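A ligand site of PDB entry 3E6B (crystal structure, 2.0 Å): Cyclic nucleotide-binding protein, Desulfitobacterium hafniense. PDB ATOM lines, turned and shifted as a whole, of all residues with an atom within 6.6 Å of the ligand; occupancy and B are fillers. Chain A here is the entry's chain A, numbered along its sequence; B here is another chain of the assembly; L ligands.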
ATOM      1  N   PHE A  19      24.778 -13.203  23.386  1.00  0.00           N
ATOM      2  CA  PHE A  19      23.753 -12.505  24.140  1.00  0.00           C
ATOM      3  C   PHE A  19      24.270 -12.055  25.469  1.00  0.00           C
ATOM      4  O   PHE A  19      24.911 -12.865  26.214  1.00  0.00           O
ATOM      5  CB  PHE A  19      22.511 -13.349  24.347  1.00  0.00           C
ATOM      6  CG  PHE A  19      21.553 -13.228  23.239  1.00  0.00           C
ATOM      7  CD1 PHE A  19      21.020 -11.992  22.905  1.00  0.00           C
ATOM      8  CD2 PHE A  19      21.184 -14.355  22.498  1.00  0.00           C
ATOM      9  CE1 PHE A  19      20.147 -11.873  21.878  1.00  0.00           C
ATOM     10  CE2 PHE A  19      20.292 -14.227  21.457  1.00  0.00           C
ATOM     11  CZ  PHE A  19      19.780 -12.981  21.159  1.00  0.00           C
ATOM     12  N   LEU A  63      22.785 -24.162  19.546  1.00  0.00           N
ATOM     13  CA  LEU A  63      21.498 -24.471  20.121  1.00  0.00           C
ATOM     14  C   LEU A  63      20.417 -24.392  19.033  1.00  0.00           C
ATOM     15  O   LEU A  63      20.288 -23.369  18.363  1.00  0.00           O
ATOM     16  CB  LEU A  63      21.247 -23.467  21.267  1.00  0.00           C
ATOM     17  CG  LEU A  63      20.160 -23.715  22.316  1.00  0.00           C
ATOM     18  CD1 LEU A  63      20.540 -23.109  23.683  1.00  0.00           C
ATOM     19  CD2 LEU A  63      18.832 -23.130  21.805  1.00  0.00           C
ATOM     20  N   ILE A  65      16.217 -25.488  17.778  1.00  0.00           N
ATOM     21  CA  ILE A  65      14.853 -25.913  18.096  1.00  0.00           C
ATOM     22  C   ILE A  65      14.484 -27.067  17.156  1.00  0.00           C
ATOM     23  O   ILE A  65      14.925 -27.102  15.993  1.00  0.00           O
ATOM     24  CB  ILE A  65      13.798 -24.762  17.997  1.00  0.00           C
ATOM     25  CG1 ILE A  65      14.129 -23.603  18.919  1.00  0.00           C
ATOM     26  CG2 ILE A  65      12.388 -25.240  18.371  1.00  0.00           C
ATOM     27  CD1 ILE A  65      12.948 -22.641  19.162  1.00  0.00           C
ATOM     28  N   LEU A  75      18.762 -21.591  16.496  1.00  0.00           N
ATOM     29  CA  LEU A  75      18.308 -20.454  17.281  1.00  0.00           C
ATOM     30  C   LEU A  75      19.501 -19.525  17.485  1.00  0.00           C
ATOM     31  O   LEU A  75      19.484 -18.349  17.074  1.00  0.00           O
ATOM     32  CB  LEU A  75      17.768 -20.936  18.623  1.00  0.00           C
ATOM     33  CG  LEU A  75      16.373 -20.489  19.040  1.00  0.00           C
ATOM     34  CD1 LEU A  75      16.195 -20.628  20.562  1.00  0.00           C
ATOM     35  CD2 LEU A  75      16.147 -19.052  18.600  1.00  0.00           C
ATOM     36  N   TYR A  76      20.539 -20.047  18.124  1.00  0.00           N
ATOM     37  CA  TYR A  76      21.722 -19.237  18.271  1.00  0.00           C
ATOM     38  C   TYR A  76      22.968 -20.042  18.523  1.00  0.00           C
ATOM     39  O   TYR A  76      22.910 -21.214  18.856  1.00  0.00           O
ATOM     40  CB  TYR A  76      21.560 -18.152  19.342  1.00  0.00           C
ATOM     41  CG  TYR A  76      21.361 -18.606  20.804  1.00  0.00           C
ATOM     42  CD1 TYR A  76      20.123 -18.454  21.451  1.00  0.00           C
ATOM     43  CD2 TYR A  76      22.431 -19.149  21.541  1.00  0.00           C
ATOM     44  CE1 TYR A  76      19.953 -18.825  22.825  1.00  0.00           C
ATOM     45  CE2 TYR A  76      22.265 -19.529  22.905  1.00  0.00           C
ATOM     46  CZ  TYR A  76      21.027 -19.356  23.533  1.00  0.00           C
ATOM     47  OH  TYR A  76      20.893 -19.738  24.852  1.00  0.00           O
ATOM     48  N   LEU A  83      24.792 -17.185  28.477  1.00  0.00           N
ATOM     49  CA  LEU A  83      23.834 -17.827  29.367  1.00  0.00           C
ATOM     50  C   LEU A  83      22.706 -18.458  28.572  1.00  0.00           C
ATOM     51  O   LEU A  83      22.114 -17.824  27.695  1.00  0.00           O
ATOM     52  CB  LEU A  83      23.280 -16.803  30.376  1.00  0.00           C
ATOM     53  CG  LEU A  83      22.436 -17.334  31.541  1.00  0.00           C
ATOM     54  CD1 LEU A  83      23.226 -18.322  32.423  1.00  0.00           C
ATOM     55  CD2 LEU A  83      21.913 -16.150  32.367  1.00  0.00           C
ATOM     56  N   ILE A  84      22.457 -19.730  28.851  1.00  0.00           N
ATOM     57  CA  ILE A  84      21.275 -20.452  28.343  1.00  0.00           C
ATOM     58  C   ILE A  84      20.226 -20.384  29.466  1.00  0.00           C
ATOM     59  O   ILE A  84      20.408 -20.998  30.521  1.00  0.00           O
ATOM     60  CB  ILE A  84      21.603 -21.953  27.922  1.00  0.00           C
ATOM     61  CG1 ILE A  84      22.753 -21.989  26.877  1.00  0.00           C
ATOM     62  CG2 ILE A  84      20.366 -22.685  27.432  1.00  0.00           C
ATOM     63  CD1 ILE A  84      23.396 -23.384  26.724  1.00  0.00           C
ATOM     64  N   GLY A  85      19.162 -19.592  29.242  1.00  0.00           N
ATOM     65  CA  GLY A  85      18.194 -19.211  30.304  1.00  0.00           C
ATOM     66  C   GLY A  85      17.019 -20.159  30.556  1.00  0.00           C
ATOM     67  O   GLY A  85      15.937 -19.724  31.021  1.00  0.00           O
ATOM     68  N   LYS A  86      17.254 -21.443  30.303  1.00  0.00           N
ATOM     69  CA  LYS A  86      16.236 -22.521  30.329  1.00  0.00           C
ATOM     70  C   LYS A  86      15.957 -23.135  31.704  1.00  0.00           C
ATOM     71  O   LYS A  86      15.999 -24.373  31.918  1.00  0.00           O
ATOM     72  CB  LYS A  86      16.613 -23.637  29.332  1.00  0.00           C
ATOM     73  CG  LYS A  86      16.565 -23.176  27.899  1.00  0.00           C
ATOM     74  CD  LYS A  86      16.956 -24.306  26.853  1.00  0.00           C
ATOM     75  CE  LYS A  86      16.070 -25.543  26.993  1.00  0.00           C
ATOM     76  NZ  LYS A  86      14.543 -25.439  27.055  1.00  0.00           N
ATOM     77  N   TYR A  88      13.177 -23.169  33.304  1.00  0.00           N
ATOM     78  CA  TYR A  88      11.878 -23.851  33.382  1.00  0.00           C
ATOM     79  C   TYR A  88      11.452 -24.435  32.018  1.00  0.00           C
ATOM     80  O   TYR A  88      12.011 -24.023  30.992  1.00  0.00           O
ATOM     81  CB  TYR A  88      10.817 -22.867  33.892  1.00  0.00           C
ATOM     82  CG  TYR A  88      11.159 -22.224  35.224  1.00  0.00           C
ATOM     83  CD1 TYR A  88      11.598 -20.904  35.291  1.00  0.00           C
ATOM     84  CD2 TYR A  88      11.067 -22.965  36.420  1.00  0.00           C
ATOM     85  CE1 TYR A  88      11.942 -20.342  36.491  1.00  0.00           C
ATOM     86  CE2 TYR A  88      11.378 -22.399  37.624  1.00  0.00           C
ATOM     87  CZ  TYR A  88      11.817 -21.098  37.658  1.00  0.00           C
ATOM     88  OH  TYR A  88      12.121 -20.543  38.858  1.00  0.00           O
ATOM     89  N   PRO A  89      10.478 -25.391  32.004  1.00  0.00           N
ATOM     90  CA  PRO A  89       9.858 -25.872  30.731  1.00  0.00           C
ATOM     91  C   PRO A  89       9.262 -24.762  29.874  1.00  0.00           C
ATOM     92  O   PRO A  89       8.570 -23.850  30.407  1.00  0.00           O
ATOM     93  CB  PRO A  89       8.751 -26.844  31.191  1.00  0.00           C
ATOM     94  CG  PRO A  89       8.687 -26.728  32.684  1.00  0.00           C
ATOM     95  CD  PRO A  89       9.963 -26.121  33.180  1.00  0.00           C
ATOM     96  N   THR A  90       9.518 -24.849  28.562  1.00  0.00           N
ATOM     97  CA  THR A  90       9.180 -23.779  27.604  1.00  0.00           C
ATOM     98  C   THR A  90       8.206 -24.159  26.489  1.00  0.00           C
ATOM     99  O   THR A  90       7.627 -23.266  25.870  1.00  0.00           O
ATOM    100  CB  THR A  90      10.420 -23.154  26.898  1.00  0.00           C
ATOM    101  OG1 THR A  90      10.912 -24.067  25.898  1.00  0.00           O
ATOM    102  CG2 THR A  90      11.549 -22.781  27.892  1.00  0.00           C
ATOM    103  N   GLY A  91       8.052 -25.445  26.211  1.00  0.00           N
ATOM    104  CA  GLY A  91       7.209 -25.831  25.073  1.00  0.00           C
ATOM    105  C   GLY A  91       7.998 -25.972  23.781  1.00  0.00           C
ATOM    106  O   GLY A  91       7.505 -26.555  22.824  1.00  0.00           O
ATOM    107  N   ASN A  92       9.228 -25.467  23.751  1.00  0.00           N
ATOM    108  CA  ASN A  92      10.154 -25.710  22.643  1.00  0.00           C
ATOM    109  C   ASN A  92      11.032 -26.894  22.936  1.00  0.00           C
ATOM    110  O   ASN A  92      11.625 -26.992  23.996  1.00  0.00           O
ATOM    111  CB  ASN A  92      11.044 -24.514  22.385  1.00  0.00           C
ATOM    112  CG  ASN A  92      10.289 -23.321  21.832  1.00  0.00           C
ATOM    113  OD1 ASN A  92       9.403 -23.492  20.997  1.00  0.00           O
ATOM    114  ND2 ASN A  92      10.636 -22.096  22.301  1.00  0.00           N
ATOM    115  N   ASN A  93      11.153 -27.801  21.968  1.00  0.00           N
ATOM    116  CA  ASN A  93      12.036 -28.952  22.091  1.00  0.00           C
ATOM    117  C   ASN A  93      13.429 -28.511  21.636  1.00  0.00           C
ATOM    118  O   ASN A  93      13.649 -28.188  20.474  1.00  0.00           O
ATOM    119  CB  ASN A  93      11.459 -30.106  21.238  1.00  0.00           C
ATOM    120  CG  ASN A  93      12.252 -31.414  21.354  1.00  0.00           C
ATOM    121  OD1 ASN A  93      13.249 -31.500  22.062  1.00  0.00           O
ATOM    122  ND2 ASN A  93      11.796 -32.434  20.605  1.00  0.00           N
ATOM    123  N   ILE A  94      14.373 -28.499  22.549  1.00  0.00           N
ATOM    124  CA  ILE A  94      15.689 -27.923  22.288  1.00  0.00           C
ATOM    125  C   ILE A  94      16.761 -28.988  22.216  1.00  0.00           C
ATOM    126  O   ILE A  94      16.724 -30.011  22.930  1.00  0.00           O
ATOM    127  CB  ILE A  94      16.087 -26.846  23.371  1.00  0.00           C
ATOM    128  CG1 ILE A  94      15.057 -25.713  23.440  1.00  0.00           C
ATOM    129  CG2 ILE A  94      17.471 -26.289  23.103  1.00  0.00           C
ATOM    130  CD1 ILE A  94      15.210 -24.672  22.321  1.00  0.00           C
ATOM    131  N   ASN A 129      20.148  -9.902  30.544  1.00  0.00           N
ATOM    132  CA  ASN A 129      20.396 -10.909  29.582  1.00  0.00           C
ATOM    133  C   ASN A 129      19.075 -11.377  28.885  1.00  0.00           C
ATOM    134  O   ASN A 129      19.012 -11.432  27.670  1.00  0.00           O
ATOM    135  CB  ASN A 129      21.100 -12.100  30.258  1.00  0.00           C
ATOM    136  CG  ASN A 129      21.563 -13.159  29.257  1.00  0.00           C
ATOM    137  OD1 ASN A 129      20.896 -14.160  29.029  1.00  0.00           O
ATOM    138  ND2 ASN A 129      22.729 -12.963  28.694  1.00  0.00           N
ATOM    139  N   TYR A 130      18.071 -11.755  29.670  1.00  0.00           N
ATOM    140  CA  TYR A 130      16.744 -12.092  29.131  1.00  0.00           C
ATOM    141  C   TYR A 130      16.178 -10.959  28.304  1.00  0.00           C
ATOM    142  O   TYR A 130      15.675 -11.168  27.200  1.00  0.00           O
ATOM    143  CB  TYR A 130      15.764 -12.430  30.266  1.00  0.00           C
ATOM    144  CG  TYR A 130      15.755 -13.842  30.800  1.00  0.00           C
ATOM    145  CD1 TYR A 130      15.471 -14.937  29.947  1.00  0.00           C
ATOM    146  CD2 TYR A 130      15.857 -14.087  32.177  1.00  0.00           C
ATOM    147  CE1 TYR A 130      15.378 -16.283  30.490  1.00  0.00           C
ATOM    148  CE2 TYR A 130      15.794 -15.438  32.726  1.00  0.00           C
ATOM    149  CZ  TYR A 130      15.557 -16.494  31.867  1.00  0.00           C
ATOM    150  OH  TYR A 130      15.461 -17.749  32.409  1.00  0.00           O
ATOM    151  N   LYS A 133      17.683 -10.660  24.839  1.00  0.00           N
ATOM    152  CA  LYS A 133      17.130 -11.698  23.984  1.00  0.00           C
ATOM    153  C   LYS A 133      15.701 -11.365  23.495  1.00  0.00           C
ATOM    154  O   LYS A 133      15.381 -11.650  22.320  1.00  0.00           O
ATOM    155  CB  LYS A 133      17.133 -13.043  24.734  1.00  0.00           C
ATOM    156  CG  LYS A 133      18.522 -13.619  24.982  1.00  0.00           C
ATOM    157  CD  LYS A 133      18.403 -14.945  25.882  1.00  0.00           C
ATOM    158  CE  LYS A 133      19.780 -15.512  26.261  1.00  0.00           C
ATOM    159  NZ  LYS A 133      19.575 -16.710  27.177  1.00  0.00           N
ATOM    160  N   TYR B 130       9.963 -13.586  31.470  1.00  0.00           N
ATOM    161  CA  TYR B 130      10.931 -13.299  30.461  1.00  0.00           C
ATOM    162  C   TYR B 130      11.145 -14.507  29.511  1.00  0.00           C
ATOM    163  O   TYR B 130      11.186 -14.322  28.314  1.00  0.00           O
ATOM    164  CB  TYR B 130      12.278 -12.890  31.044  1.00  0.00           C
ATOM    165  CG  TYR B 130      12.522 -11.404  31.302  1.00  0.00           C
ATOM    166  CD1 TYR B 130      12.528 -10.453  30.243  1.00  0.00           C
ATOM    167  CD2 TYR B 130      12.853 -10.963  32.589  1.00  0.00           C
ATOM    168  CE1 TYR B 130      12.786  -9.097  30.521  1.00  0.00           C
ATOM    169  CE2 TYR B 130      13.141  -9.642  32.849  1.00  0.00           C
ATOM    170  CZ  TYR B 130      13.097  -8.692  31.830  1.00  0.00           C
ATOM    171  OH  TYR B 130      13.378  -7.356  32.153  1.00  0.00           O
ATOM    172  N   LEU B 131      11.337 -15.686  30.105  1.00  0.00           N
ATOM    173  CA  LEU B 131      11.617 -16.910  29.405  1.00  0.00           C
ATOM    174  C   LEU B 131      10.434 -17.265  28.452  1.00  0.00           C
ATOM    175  O   LEU B 131      10.669 -17.642  27.320  1.00  0.00           O
ATOM    176  CB  LEU B 131      11.909 -18.031  30.409  1.00  0.00           C
ATOM    177  CG  LEU B 131      12.013 -19.443  29.783  1.00  0.00           C
ATOM    178  CD1 LEU B 131      13.256 -19.451  28.854  1.00  0.00           C
ATOM    179  CD2 LEU B 131      12.127 -20.477  30.870  1.00  0.00           C
ATOM    180  N   VAL B 134      10.961 -15.023  25.363  1.00  0.00           N
ATOM    181  CA  VAL B 134      12.055 -15.426  24.482  1.00  0.00           C
ATOM    182  C   VAL B 134      11.592 -16.709  23.712  1.00  0.00           C
ATOM    183  O   VAL B 134      11.891 -16.858  22.516  1.00  0.00           O
ATOM    184  CB  VAL B 134      13.390 -15.735  25.262  1.00  0.00           C
ATOM    185  CG1 VAL B 134      14.517 -16.321  24.316  1.00  0.00           C
ATOM    186  CG2 VAL B 134      13.940 -14.509  26.055  1.00  0.00           C
ATOM    187  N   ALA B 135      10.875 -17.602  24.402  1.00  0.00           N
ATOM    188  CA  ALA B 135      10.478 -18.881  23.875  1.00  0.00           C
ATOM    189  C   ALA B 135       9.516 -18.666  22.725  1.00  0.00           C
ATOM    190  O   ALA B 135       9.613 -19.339  21.704  1.00  0.00           O
ATOM    191  CB  ALA B 135       9.842 -19.757  24.956  1.00  0.00           C
ATOM    192  N   TYR B 136       8.610 -17.692  22.897  1.00  0.00           N
ATOM    193  CA  TYR B 136       7.645 -17.303  21.868  1.00  0.00           C
ATOM    194  C   TYR B 136       8.240 -16.635  20.611  1.00  0.00           C
ATOM    195  O   TYR B 136       7.924 -17.053  19.464  1.00  0.00           O
ATOM    196  CB  TYR B 136       6.550 -16.404  22.484  1.00  0.00           C
ATOM    197  CG  TYR B 136       5.582 -15.934  21.454  1.00  0.00           C
ATOM    198  CD1 TYR B 136       4.475 -16.708  21.142  1.00  0.00           C
ATOM    199  CD2 TYR B 136       5.757 -14.728  20.790  1.00  0.00           C
ATOM    200  CE1 TYR B 136       3.574 -16.292  20.172  1.00  0.00           C
ATOM    201  CE2 TYR B 136       4.858 -14.322  19.819  1.00  0.00           C
ATOM    202  CZ  TYR B 136       3.781 -15.113  19.523  1.00  0.00           C
ATOM    203  OH  TYR B 136       2.870 -14.741  18.577  1.00  0.00           O
ATOM    204  N   ALA B 138      11.565 -16.487  19.701  1.00  0.00           N
ATOM    205  CA  ALA B 138      12.609 -17.328  19.132  1.00  0.00           C
ATOM    206  C   ALA B 138      12.050 -18.458  18.275  1.00  0.00           C
ATOM    207  O   ALA B 138      12.658 -18.802  17.260  1.00  0.00           O
ATOM    208  CB  ALA B 138      13.493 -17.887  20.216  1.00  0.00           C
HETATM  209  O1  LIG L   1      12.325 -22.657  24.452  1.00  0.00           O
HETATM  210  C1  LIG L   1      13.479 -22.404  24.768  1.00  0.00           C
HETATM  211  O2  LIG L   1      14.097 -23.168  25.534  1.00  0.00           O
HETATM  212  C2  LIG L   1      14.042 -21.121  24.210  1.00  0.00           C
HETATM  213  C3  LIG L   1      15.321 -20.572  24.814  1.00  0.00           C
HETATM  214  C4  LIG L   1      16.529 -21.091  24.398  1.00  0.00           C
HETATM  215  C5  LIG L   1      17.654 -20.670  24.861  1.00  0.00           C
HETATM  216  C6  LIG L   1      17.740 -19.546  25.828  1.00  0.00           C
HETATM  217  O3  LIG L   1      18.930 -18.998  26.370  1.00  0.00           O
HETATM  218 CL1  LIG L   1      16.360 -17.775  27.382  1.00  0.00          CL
HETATM  219  C7  LIG L   1      16.384 -19.051  26.228  1.00  0.00           C
HETATM  220  C8  LIG L   1      15.254 -19.560  25.713  1.00  0.00           C
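CD1 of Leu 63 touches C5 of the ligand (3.96 Å).
Leu 75 touches the ligand.
Leu 83 touches the ligand (O to O3, 3.6 Å).
CA of Ile 84 touches O3 of the ligand (3.4 Å).
Ile 94 touches the ligand.
Tyr 130 of chain A touches the ligand (CE1 to CL1, 3.6 Å).
Leu 131 of chain B touches the ligand (CD1 to C8, 3.7 Å).
CG1 of Val 134 of chain B touches C8 of the ligand, 3.6 Å away.
Ala 135 of chain B touches the ligand.
Hydrophobic or aromatic side chains that line the ligand: Leu 63, Leu 75, Tyr 76, Ile 94, Tyr 130 of chain A, Leu 131 of chain B, Val 134 of chain B and Ala 135 of chain B.
Of the 25 residues printed, 15 come within 4 Å of the ligand.
The nearest printed residue that does not touch the ligand is Ala 138 of chain B (5.2 Å).
An oxygen (O1) of the ligand sits at hydrogen-bond distance from the side-chain hydroxyl (OG1) of Thr 90, at 2.5 Å.
The side-chain amino group (NZ) of Lys 133 sits at hydrogen-bond distance from an oxygen (O3) of the ligand (2.5 Å).
The side-chain hydroxyl (OH) of Tyr 76 lies within hydrogen-bond range of an oxygen (O3) of the ligand (2.6 Å).
An oxygen (O2) of the ligand lies within salt-bridge range of the side-chain amino group (NZ) of Lys 86, 2.8 Å away.
ND2 of Asn 92 is in hydrogen-bond range of O1 of the ligand.
The backbone NH (N) of Gly 85 sits at hydrogen-bond distance from an oxygen (O3) of the ligand (2.9 Å).
N of Asn 92 lies within hydrogen-bond range of OG1 of Thr 90, at 3.1 Å.
The side-chain amino group (NZ) of Lys 133 lies within hydrogen-bond range of the backbone carbonyl oxygen (O) of Leu 83 (2.8 Å).
OD1 of Asn 129 sits close to NZ of Lys 133 (3.4 Å).
The backbone NH of Leu 63 lies within hydrogen-bond range of the backbone carbonyl oxygen of Tyr 76 (3.0 Å).
ND2 of Asn 92 is in hydrogen-bond range of O of Ala 135 of chain B, at 3.0 Å.
O of Gly 85 lies within hydrogen-bond range of OH of Tyr 130 of chain A, 2.5 Å away.
The backbone NH (N) of Leu 75 lies within hydrogen-bond range of the backbone carbonyl oxygen (O) of Leu 63 (3.0 Å).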
